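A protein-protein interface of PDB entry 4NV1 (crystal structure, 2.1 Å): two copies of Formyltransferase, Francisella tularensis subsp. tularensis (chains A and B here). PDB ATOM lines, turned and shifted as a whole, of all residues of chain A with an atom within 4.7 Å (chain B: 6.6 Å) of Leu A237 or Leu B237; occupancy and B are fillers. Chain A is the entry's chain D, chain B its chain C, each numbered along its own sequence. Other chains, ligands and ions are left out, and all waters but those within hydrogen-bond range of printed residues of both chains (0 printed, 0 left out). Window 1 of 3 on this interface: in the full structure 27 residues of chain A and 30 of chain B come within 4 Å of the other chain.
Printed residues of chain B within 4 Å of Ala A236: Leu B237 and Glu B238. Leu A237 touches just these residues of chain B: Ala B236 (3.5 Å) and Leu B237 (3.8 Å). Of the printed residues of chain B, Glu A238 touches Val B235 (3.3 Å) and Ala B236 (2.9 Å). Of the printed residues of chain A, Ala B236 touches Leu A237 and Glu A238. Leu B237 touches two residues of chain A. The nearest residue of chain B that does not touch Leu A237 is Leu B212 (4.1 Å). The nearest residue of chain A that does not touch Leu B237 is Leu A212 (4.1 Å).
The backbone NH (N) of Leu A237 lies within hydrogen-bond range of the side-chain hydroxyl (OG1) of Thr A216 (3.0 Å). N of Leu B237 sits at hydrogen-bond distance from OG1 of Thr B216, at 2.8 Å.
Printed residues of chain A that touch a printed residue of chain B: Val A235, Ala A236, Leu A237 and Glu A238. Hydrophobic or aromatic side chains of chain A within 4 Å of the printed part of chain B: Val A235 and Leu A237. Hydrophobic or aromatic side chains of chain B that line the printed part of chain A: Ala B236, Leu B237 and Leu B239. Among the printed residues, no Asp or Glu carboxylate lies within 4 Å of a Lys or Arg side-chain nitrogen of the other chain.
Val A235 touches Glu B238, and with the chains exchanged Glu A238 touches Val B235. Val A235 touches Leu B239, but with the chains exchanged Leu A239 does not touch Val B235 (4.2 Å). Ala A236 touches Glu B238, and with the chains exchanged Glu A238 touches Ala B236. Leu B237 touches its own counterpart, Leu A237. 9 positions are printed for both chains.
CA of Val A235 touches O of Glu B238 (3.2 Å). CD2 of Leu B239 touches CG1 of Val A235, at 3.6 Å. CD1 of Leu B237 touches O of Ala A236 (3.3 Å). O of Ala B236 touches CD1 of Leu A237 (3.5 Å). Leu A237 touches Leu B237. Glu A238 touches Val B235 (O to CA, 3.3 Å).
The backbone NH (N) of Glu A238 sits at hydrogen-bond distance from the backbone carbonyl oxygen (O) of Ala B236 (2.9 Å). The backbone carbonyl oxygen (O) of Ala A236 sits at hydrogen-bond distance from the backbone NH (N) of Glu B238 (2.7 Å).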
ATOM      1  N   ILE A 209      14.305 -34.137  12.391  1.00  0.00           N
ATOM      2  CA  ILE A 209      13.601 -33.165  13.199  1.00  0.00           C
ATOM      3  C   ILE A 209      13.847 -33.441  14.679  1.00  0.00           C
ATOM      4  O   ILE A 209      14.153 -32.532  15.428  1.00  0.00           O
ATOM      5  CB  ILE A 209      12.098 -33.238  12.886  1.00  0.00           C
ATOM      6  CG1 ILE A 209      11.872 -32.631  11.512  1.00  0.00           C
ATOM      7  CG2 ILE A 209      11.276 -32.502  13.935  1.00  0.00           C
ATOM      8  CD1 ILE A 209      10.493 -32.935  10.961  1.00  0.00           C
ATOM      9  N   LEU A 212      17.372 -32.307  15.467  1.00  0.00           N
ATOM     10  CA  LEU A 212      17.577 -30.843  15.538  1.00  0.00           C
ATOM     11  C   LEU A 212      16.855 -30.151  16.729  1.00  0.00           C
ATOM     12  O   LEU A 212      17.381 -29.193  17.305  1.00  0.00           O
ATOM     13  CB  LEU A 212      17.091 -30.256  14.215  1.00  0.00           C
ATOM     14  CG  LEU A 212      18.053 -30.491  13.027  1.00  0.00           C
ATOM     15  CD1 LEU A 212      17.391 -30.075  11.755  1.00  0.00           C
ATOM     16  CD2 LEU A 212      19.330 -29.684  13.104  1.00  0.00           C
ATOM     17  N   ARG A 213      15.676 -30.647  17.082  1.00  0.00           N
ATOM     18  CA  ARG A 213      14.944 -30.161  18.231  1.00  0.00           C
ATOM     19  C   ARG A 213      15.685 -30.571  19.517  1.00  0.00           C
ATOM     20  O   ARG A 213      15.732 -29.782  20.487  1.00  0.00           O
ATOM     21  CB  ARG A 213      13.505 -30.659  18.164  1.00  0.00           C
ATOM     22  CG  ARG A 213      13.176 -32.015  18.758  1.00  0.00           C
ATOM     23  CD  ARG A 213      11.824 -32.324  18.152  1.00  0.00           C
ATOM     24  NE  ARG A 213      11.321 -33.679  18.355  1.00  0.00           N
ATOM     25  CZ  ARG A 213      10.548 -34.044  19.369  1.00  0.00           C
ATOM     26  NH1 ARG A 213      10.209 -33.230  20.372  1.00  0.00           N
ATOM     27  NH2 ARG A 213      10.091 -35.261  19.362  1.00  0.00           N
ATOM     28  N   THR A 216      18.368 -28.086  20.028  1.00  0.00           N
ATOM     29  CA  THR A 216      17.971 -26.715  20.253  1.00  0.00           C
ATOM     30  C   THR A 216      17.753 -26.360  21.694  1.00  0.00           C
ATOM     31  O   THR A 216      16.801 -26.825  22.326  1.00  0.00           O
ATOM     32  CB  THR A 216      16.776 -26.352  19.345  1.00  0.00           C
ATOM     33  OG1 THR A 216      17.175 -26.631  17.995  1.00  0.00           O
ATOM     34  CG2 THR A 216      16.362 -24.906  19.466  1.00  0.00           C
ATOM     35  N   VAL A 235      23.013 -24.710  13.604  1.00  0.00           N
ATOM     36  CA  VAL A 235      21.623 -24.824  13.171  1.00  0.00           C
ATOM     37  C   VAL A 235      20.762 -25.084  14.426  1.00  0.00           C
ATOM     38  O   VAL A 235      21.182 -25.768  15.365  1.00  0.00           O
ATOM     39  CB  VAL A 235      21.387 -25.899  12.097  1.00  0.00           C
ATOM     40  CG1 VAL A 235      22.492 -25.846  11.045  1.00  0.00           C
ATOM     41  CG2 VAL A 235      21.423 -27.272  12.679  1.00  0.00           C
ATOM     42  N   ALA A 236      19.570 -24.538  14.431  1.00  0.00           N
ATOM     43  CA  ALA A 236      18.585 -24.794  15.496  1.00  0.00           C
ATOM     44  C   ALA A 236      17.274 -24.812  14.803  1.00  0.00           C
ATOM     45  O   ALA A 236      17.186 -24.232  13.700  1.00  0.00           O
ATOM     46  CB  ALA A 236      18.637 -23.684  16.546  1.00  0.00           C
ATOM     47  N   LEU A 237      16.280 -25.473  15.423  1.00  0.00           N
ATOM     48  CA  LEU A 237      14.929 -25.585  14.908  1.00  0.00           C
ATOM     49  C   LEU A 237      13.891 -24.917  15.808  1.00  0.00           C
ATOM     50  O   LEU A 237      14.021 -24.933  16.996  1.00  0.00           O
ATOM     51  CB  LEU A 237      14.532 -27.042  14.844  1.00  0.00           C
ATOM     52  CG  LEU A 237      13.361 -27.471  13.953  1.00  0.00           C
ATOM     53  CD1 LEU A 237      13.638 -27.480  12.449  1.00  0.00           C
ATOM     54  CD2 LEU A 237      12.956 -28.901  14.298  1.00  0.00           C
ATOM     55  N   GLU A 238      12.836 -24.389  15.227  1.00  0.00           N
ATOM     56  CA  GLU A 238      11.735 -23.775  15.933  1.00  0.00           C
ATOM     57  C   GLU A 238      10.529 -24.651  15.592  1.00  0.00           C
ATOM     58  O   GLU A 238      10.336 -25.035  14.437  1.00  0.00           O
ATOM     59  CB  GLU A 238      11.583 -22.341  15.437  1.00  0.00           C
ATOM     60  CG  GLU A 238      10.540 -21.516  16.192  1.00  0.00           C
ATOM     61  CD  GLU A 238       9.967 -20.360  15.370  1.00  0.00           C
ATOM     62  OE1 GLU A 238      10.035 -19.226  15.894  1.00  0.00           O
ATOM     63  OE2 GLU A 238       9.466 -20.574  14.225  1.00  0.00           O
ATOM     64  N   LEU A 239       9.732 -25.001  16.591  1.00  0.00           N
ATOM     65  CA  LEU A 239       8.481 -25.664  16.326  1.00  0.00           C
ATOM     66  C   LEU A 239       7.340 -24.900  16.980  1.00  0.00           C
ATOM     67  O   LEU A 239       7.535 -24.232  17.988  1.00  0.00           O
ATOM     68  CB  LEU A 239       8.547 -27.090  16.865  1.00  0.00           C
ATOM     69  CG  LEU A 239       9.812 -27.848  16.430  1.00  0.00           C
ATOM     70  CD1 LEU A 239      10.823 -27.971  17.570  1.00  0.00           C
ATOM     71  CD2 LEU A 239       9.460 -29.255  15.977  1.00  0.00           C
ATOM     72  N   ASN B 146      18.290 -18.981   4.192  1.00  0.00           N
ATOM     73  CA  ASN B 146      16.967 -19.514   4.007  1.00  0.00           C
ATOM     74  C   ASN B 146      16.226 -18.811   2.847  1.00  0.00           C
ATOM     75  O   ASN B 146      16.781 -17.944   2.157  1.00  0.00           O
ATOM     76  CB  ASN B 146      16.190 -19.385   5.348  1.00  0.00           C
ATOM     77  CG  ASN B 146      16.038 -17.944   5.799  1.00  0.00           C
ATOM     78  OD1 ASN B 146      16.051 -17.018   4.991  1.00  0.00           O
ATOM     79  ND2 ASN B 146      15.934 -17.736   7.122  1.00  0.00           N
ATOM     80  N   ALA B 208      17.390 -32.606   4.397  1.00  0.00           N
ATOM     81  CA  ALA B 208      16.380 -32.191   5.375  1.00  0.00           C
ATOM     82  C   ALA B 208      16.639 -30.743   5.649  1.00  0.00           C
ATOM     83  O   ALA B 208      15.714 -29.952   5.721  1.00  0.00           O
ATOM     84  CB  ALA B 208      16.440 -33.024   6.666  1.00  0.00           C
ATOM     85  N   ILE B 209      17.911 -30.415   5.812  1.00  0.00           N
ATOM     86  CA  ILE B 209      18.301 -29.059   6.074  1.00  0.00           C
ATOM     87  C   ILE B 209      17.954 -28.111   4.924  1.00  0.00           C
ATOM     88  O   ILE B 209      17.429 -27.006   5.162  1.00  0.00           O
ATOM     89  CB  ILE B 209      19.767 -28.992   6.477  1.00  0.00           C
ATOM     90  CG1 ILE B 209      19.836 -29.541   7.883  1.00  0.00           C
ATOM     91  CG2 ILE B 209      20.304 -27.570   6.391  1.00  0.00           C
ATOM     92  CD1 ILE B 209      21.248 -29.875   8.295  1.00  0.00           C
ATOM     93  N   ASP B 210      18.259 -28.531   3.702  1.00  0.00           N
ATOM     94  CA  ASP B 210      17.941 -27.734   2.501  1.00  0.00           C
ATOM     95  C   ASP B 210      16.447 -27.609   2.434  1.00  0.00           C
ATOM     96  O   ASP B 210      15.992 -26.498   2.299  1.00  0.00           O
ATOM     97  CB  ASP B 210      18.545 -28.293   1.214  1.00  0.00           C
ATOM     98  CG  ASP B 210      20.059 -28.123   1.179  1.00  0.00           C
ATOM     99  OD1 ASP B 210      20.645 -27.420   2.049  1.00  0.00           O
ATOM    100  OD2 ASP B 210      20.667 -28.721   0.273  1.00  0.00           O
ATOM    101  N   TYR B 211      15.693 -28.671   2.669  1.00  0.00           N
ATOM    102  CA  TYR B 211      14.246 -28.514   2.677  1.00  0.00           C
ATOM    103  C   TYR B 211      13.751 -27.510   3.778  1.00  0.00           C
ATOM    104  O   TYR B 211      12.868 -26.662   3.547  1.00  0.00           O
ATOM    105  CB  TYR B 211      13.567 -29.871   2.851  1.00  0.00           C
ATOM    106  CG  TYR B 211      12.089 -29.758   3.130  1.00  0.00           C
ATOM    107  CD1 TYR B 211      11.171 -29.690   2.109  1.00  0.00           C
ATOM    108  CD2 TYR B 211      11.619 -29.666   4.429  1.00  0.00           C
ATOM    109  CE1 TYR B 211       9.816 -29.555   2.361  1.00  0.00           C
ATOM    110  CE2 TYR B 211      10.277 -29.543   4.693  1.00  0.00           C
ATOM    111  CZ  TYR B 211       9.366 -29.453   3.667  1.00  0.00           C
ATOM    112  OH  TYR B 211       8.011 -29.298   3.937  1.00  0.00           O
ATOM    113  N   LEU B 212      14.248 -27.667   4.997  1.00  0.00           N
ATOM    114  CA  LEU B 212      13.806 -26.832   6.127  1.00  0.00           C
ATOM    115  C   LEU B 212      14.141 -25.340   5.905  1.00  0.00           C
ATOM    116  O   LEU B 212      13.302 -24.433   6.105  1.00  0.00           O
ATOM    117  CB  LEU B 212      14.407 -27.371   7.439  1.00  0.00           C
ATOM    118  CG  LEU B 212      13.694 -28.662   7.831  1.00  0.00           C
ATOM    119  CD1 LEU B 212      14.398 -29.417   8.940  1.00  0.00           C
ATOM    120  CD2 LEU B 212      12.229 -28.400   8.144  1.00  0.00           C
ATOM    121  N   ARG B 213      15.357 -25.076   5.436  1.00  0.00           N
ATOM    122  CA  ARG B 213      15.700 -23.721   5.102  1.00  0.00           C
ATOM    123  C   ARG B 213      14.951 -23.115   3.915  1.00  0.00           C
ATOM    124  O   ARG B 213      14.602 -21.902   3.943  1.00  0.00           O
ATOM    125  CB  ARG B 213      17.209 -23.483   5.066  1.00  0.00           C
ATOM    126  CG  ARG B 213      17.908 -23.970   3.791  1.00  0.00           C
ATOM    127  CD  ARG B 213      19.377 -24.150   4.039  1.00  0.00           C
ATOM    128  NE  ARG B 213      20.139 -24.748   2.946  1.00  0.00           N
ATOM    129  CZ  ARG B 213      20.910 -24.057   2.110  1.00  0.00           C
ATOM    130  NH1 ARG B 213      20.927 -22.753   2.144  1.00  0.00           N
ATOM    131  NH2 ARG B 213      21.641 -24.675   1.176  1.00  0.00           N
ATOM    132  N   MET B 215      11.915 -23.672   3.259  1.00  0.00           N
ATOM    133  CA  MET B 215      10.595 -23.375   3.797  1.00  0.00           C
ATOM    134  C   MET B 215      10.517 -22.362   4.938  1.00  0.00           C
ATOM    135  O   MET B 215       9.412 -22.106   5.440  1.00  0.00           O
ATOM    136  CB  MET B 215       9.936 -24.681   4.266  1.00  0.00           C
ATOM    137  CG  MET B 215       9.701 -25.744   3.212  1.00  0.00           C
ATOM    138  SD  MET B 215       8.606 -25.317   1.857  1.00  0.00           S
ATOM    139  CE  MET B 215       7.013 -25.590   2.567  1.00  0.00           C
ATOM    140  N   THR B 216      11.652 -21.749   5.259  1.00  0.00           N
ATOM    141  CA  THR B 216      11.798 -20.768   6.297  1.00  0.00           C
ATOM    142  C   THR B 216      11.942 -19.351   5.757  1.00  0.00           C
ATOM    143  O   THR B 216      12.911 -18.989   5.058  1.00  0.00           O
ATOM    144  CB  THR B 216      12.948 -21.113   7.287  1.00  0.00           C
ATOM    145  OG1 THR B 216      12.783 -22.452   7.808  1.00  0.00           O
ATOM    146  CG2 THR B 216      12.961 -20.115   8.417  1.00  0.00           C
ATOM    147  N   PHE B 225       4.239 -30.689  10.326  1.00  0.00           N
ATOM    148  CA  PHE B 225       3.840 -32.090  10.446  1.00  0.00           C
ATOM    149  C   PHE B 225       2.581 -32.249  11.295  1.00  0.00           C
ATOM    150  O   PHE B 225       2.227 -31.391  12.112  1.00  0.00           O
ATOM    151  CB  PHE B 225       4.955 -33.028  10.948  1.00  0.00           C
ATOM    152  CG  PHE B 225       5.504 -32.707  12.320  1.00  0.00           C
ATOM    153  CD1 PHE B 225       6.696 -32.006  12.456  1.00  0.00           C
ATOM    154  CD2 PHE B 225       4.864 -33.147  13.454  1.00  0.00           C
ATOM    155  CE1 PHE B 225       7.215 -31.683  13.684  1.00  0.00           C
ATOM    156  CE2 PHE B 225       5.400 -32.882  14.697  1.00  0.00           C
ATOM    157  CZ  PHE B 225       6.567 -32.136  14.828  1.00  0.00           C
ATOM    158  N   VAL B 235       7.315 -25.894  11.466  1.00  0.00           N
ATOM    159  CA  VAL B 235       8.715 -26.001  11.730  1.00  0.00           C
ATOM    160  C   VAL B 235       9.391 -24.925  10.929  1.00  0.00           C
ATOM    161  O   VAL B 235       8.960 -24.690   9.827  1.00  0.00           O
ATOM    162  CB  VAL B 235       9.194 -27.403  11.352  1.00  0.00           C
ATOM    163  CG1 VAL B 235       8.335 -28.445  12.022  1.00  0.00           C
ATOM    164  CG2 VAL B 235       9.116 -27.668   9.854  1.00  0.00           C
ATOM    165  N   ALA B 236      10.460 -24.330  11.444  1.00  0.00           N
ATOM    166  CA  ALA B 236      11.291 -23.331  10.779  1.00  0.00           C
ATOM    167  C   ALA B 236      12.706 -23.617  11.177  1.00  0.00           C
ATOM    168  O   ALA B 236      12.932 -24.068  12.306  1.00  0.00           O
ATOM    169  CB  ALA B 236      10.986 -21.897  11.220  1.00  0.00           C
ATOM    170  N   LEU B 237      13.673 -23.282  10.338  1.00  0.00           N
ATOM    171  CA  LEU B 237      15.043 -23.555  10.744  1.00  0.00           C
ATOM    172  C   LEU B 237      15.861 -22.307  10.923  1.00  0.00           C
ATOM    173  O   LEU B 237      15.633 -21.342  10.212  1.00  0.00           O
ATOM    174  CB  LEU B 237      15.660 -24.416   9.665  1.00  0.00           C
ATOM    175  CG  LEU B 237      17.045 -24.989   9.967  1.00  0.00           C
ATOM    176  CD1 LEU B 237      16.915 -26.124  10.965  1.00  0.00           C
ATOM    177  CD2 LEU B 237      17.628 -25.523   8.675  1.00  0.00           C
ATOM    178  N   GLU B 238      16.771 -22.266  11.879  1.00  0.00           N
ATOM    179  CA  GLU B 238      17.632 -21.133  12.040  1.00  0.00           C
ATOM    180  C   GLU B 238      19.047 -21.573  11.772  1.00  0.00           C
ATOM    181  O   GLU B 238      19.479 -22.643  12.250  1.00  0.00           O
ATOM    182  CB  GLU B 238      17.661 -20.627  13.480  1.00  0.00           C
ATOM    183  CG  GLU B 238      16.352 -20.250  14.135  1.00  0.00           C
ATOM    184  CD  GLU B 238      16.565 -20.046  15.645  1.00  0.00           C
ATOM    185  OE1 GLU B 238      17.600 -19.427  15.999  1.00  0.00           O
ATOM    186  OE2 GLU B 238      15.761 -20.537  16.473  1.00  0.00           O
ATOM    187  N   LEU B 239      19.808 -20.721  11.107  1.00  0.00           N
ATOM    188  CA  LEU B 239      21.187 -21.048  10.764  1.00  0.00           C
ATOM    189  C   LEU B 239      22.075 -19.861  11.038  1.00  0.00           C
ATOM    190  O   LEU B 239      21.736 -18.739  10.685  1.00  0.00           O
ATOM    191  CB  LEU B 239      21.313 -21.361   9.279  1.00  0.00           C
ATOM    192  CG  LEU B 239      20.421 -22.496   8.888  1.00  0.00           C
ATOM    193  CD1 LEU B 239      19.478 -22.122   7.792  1.00  0.00           C
ATOM    194  CD2 LEU B 239      21.213 -23.698   8.431  1.00  0.00           C
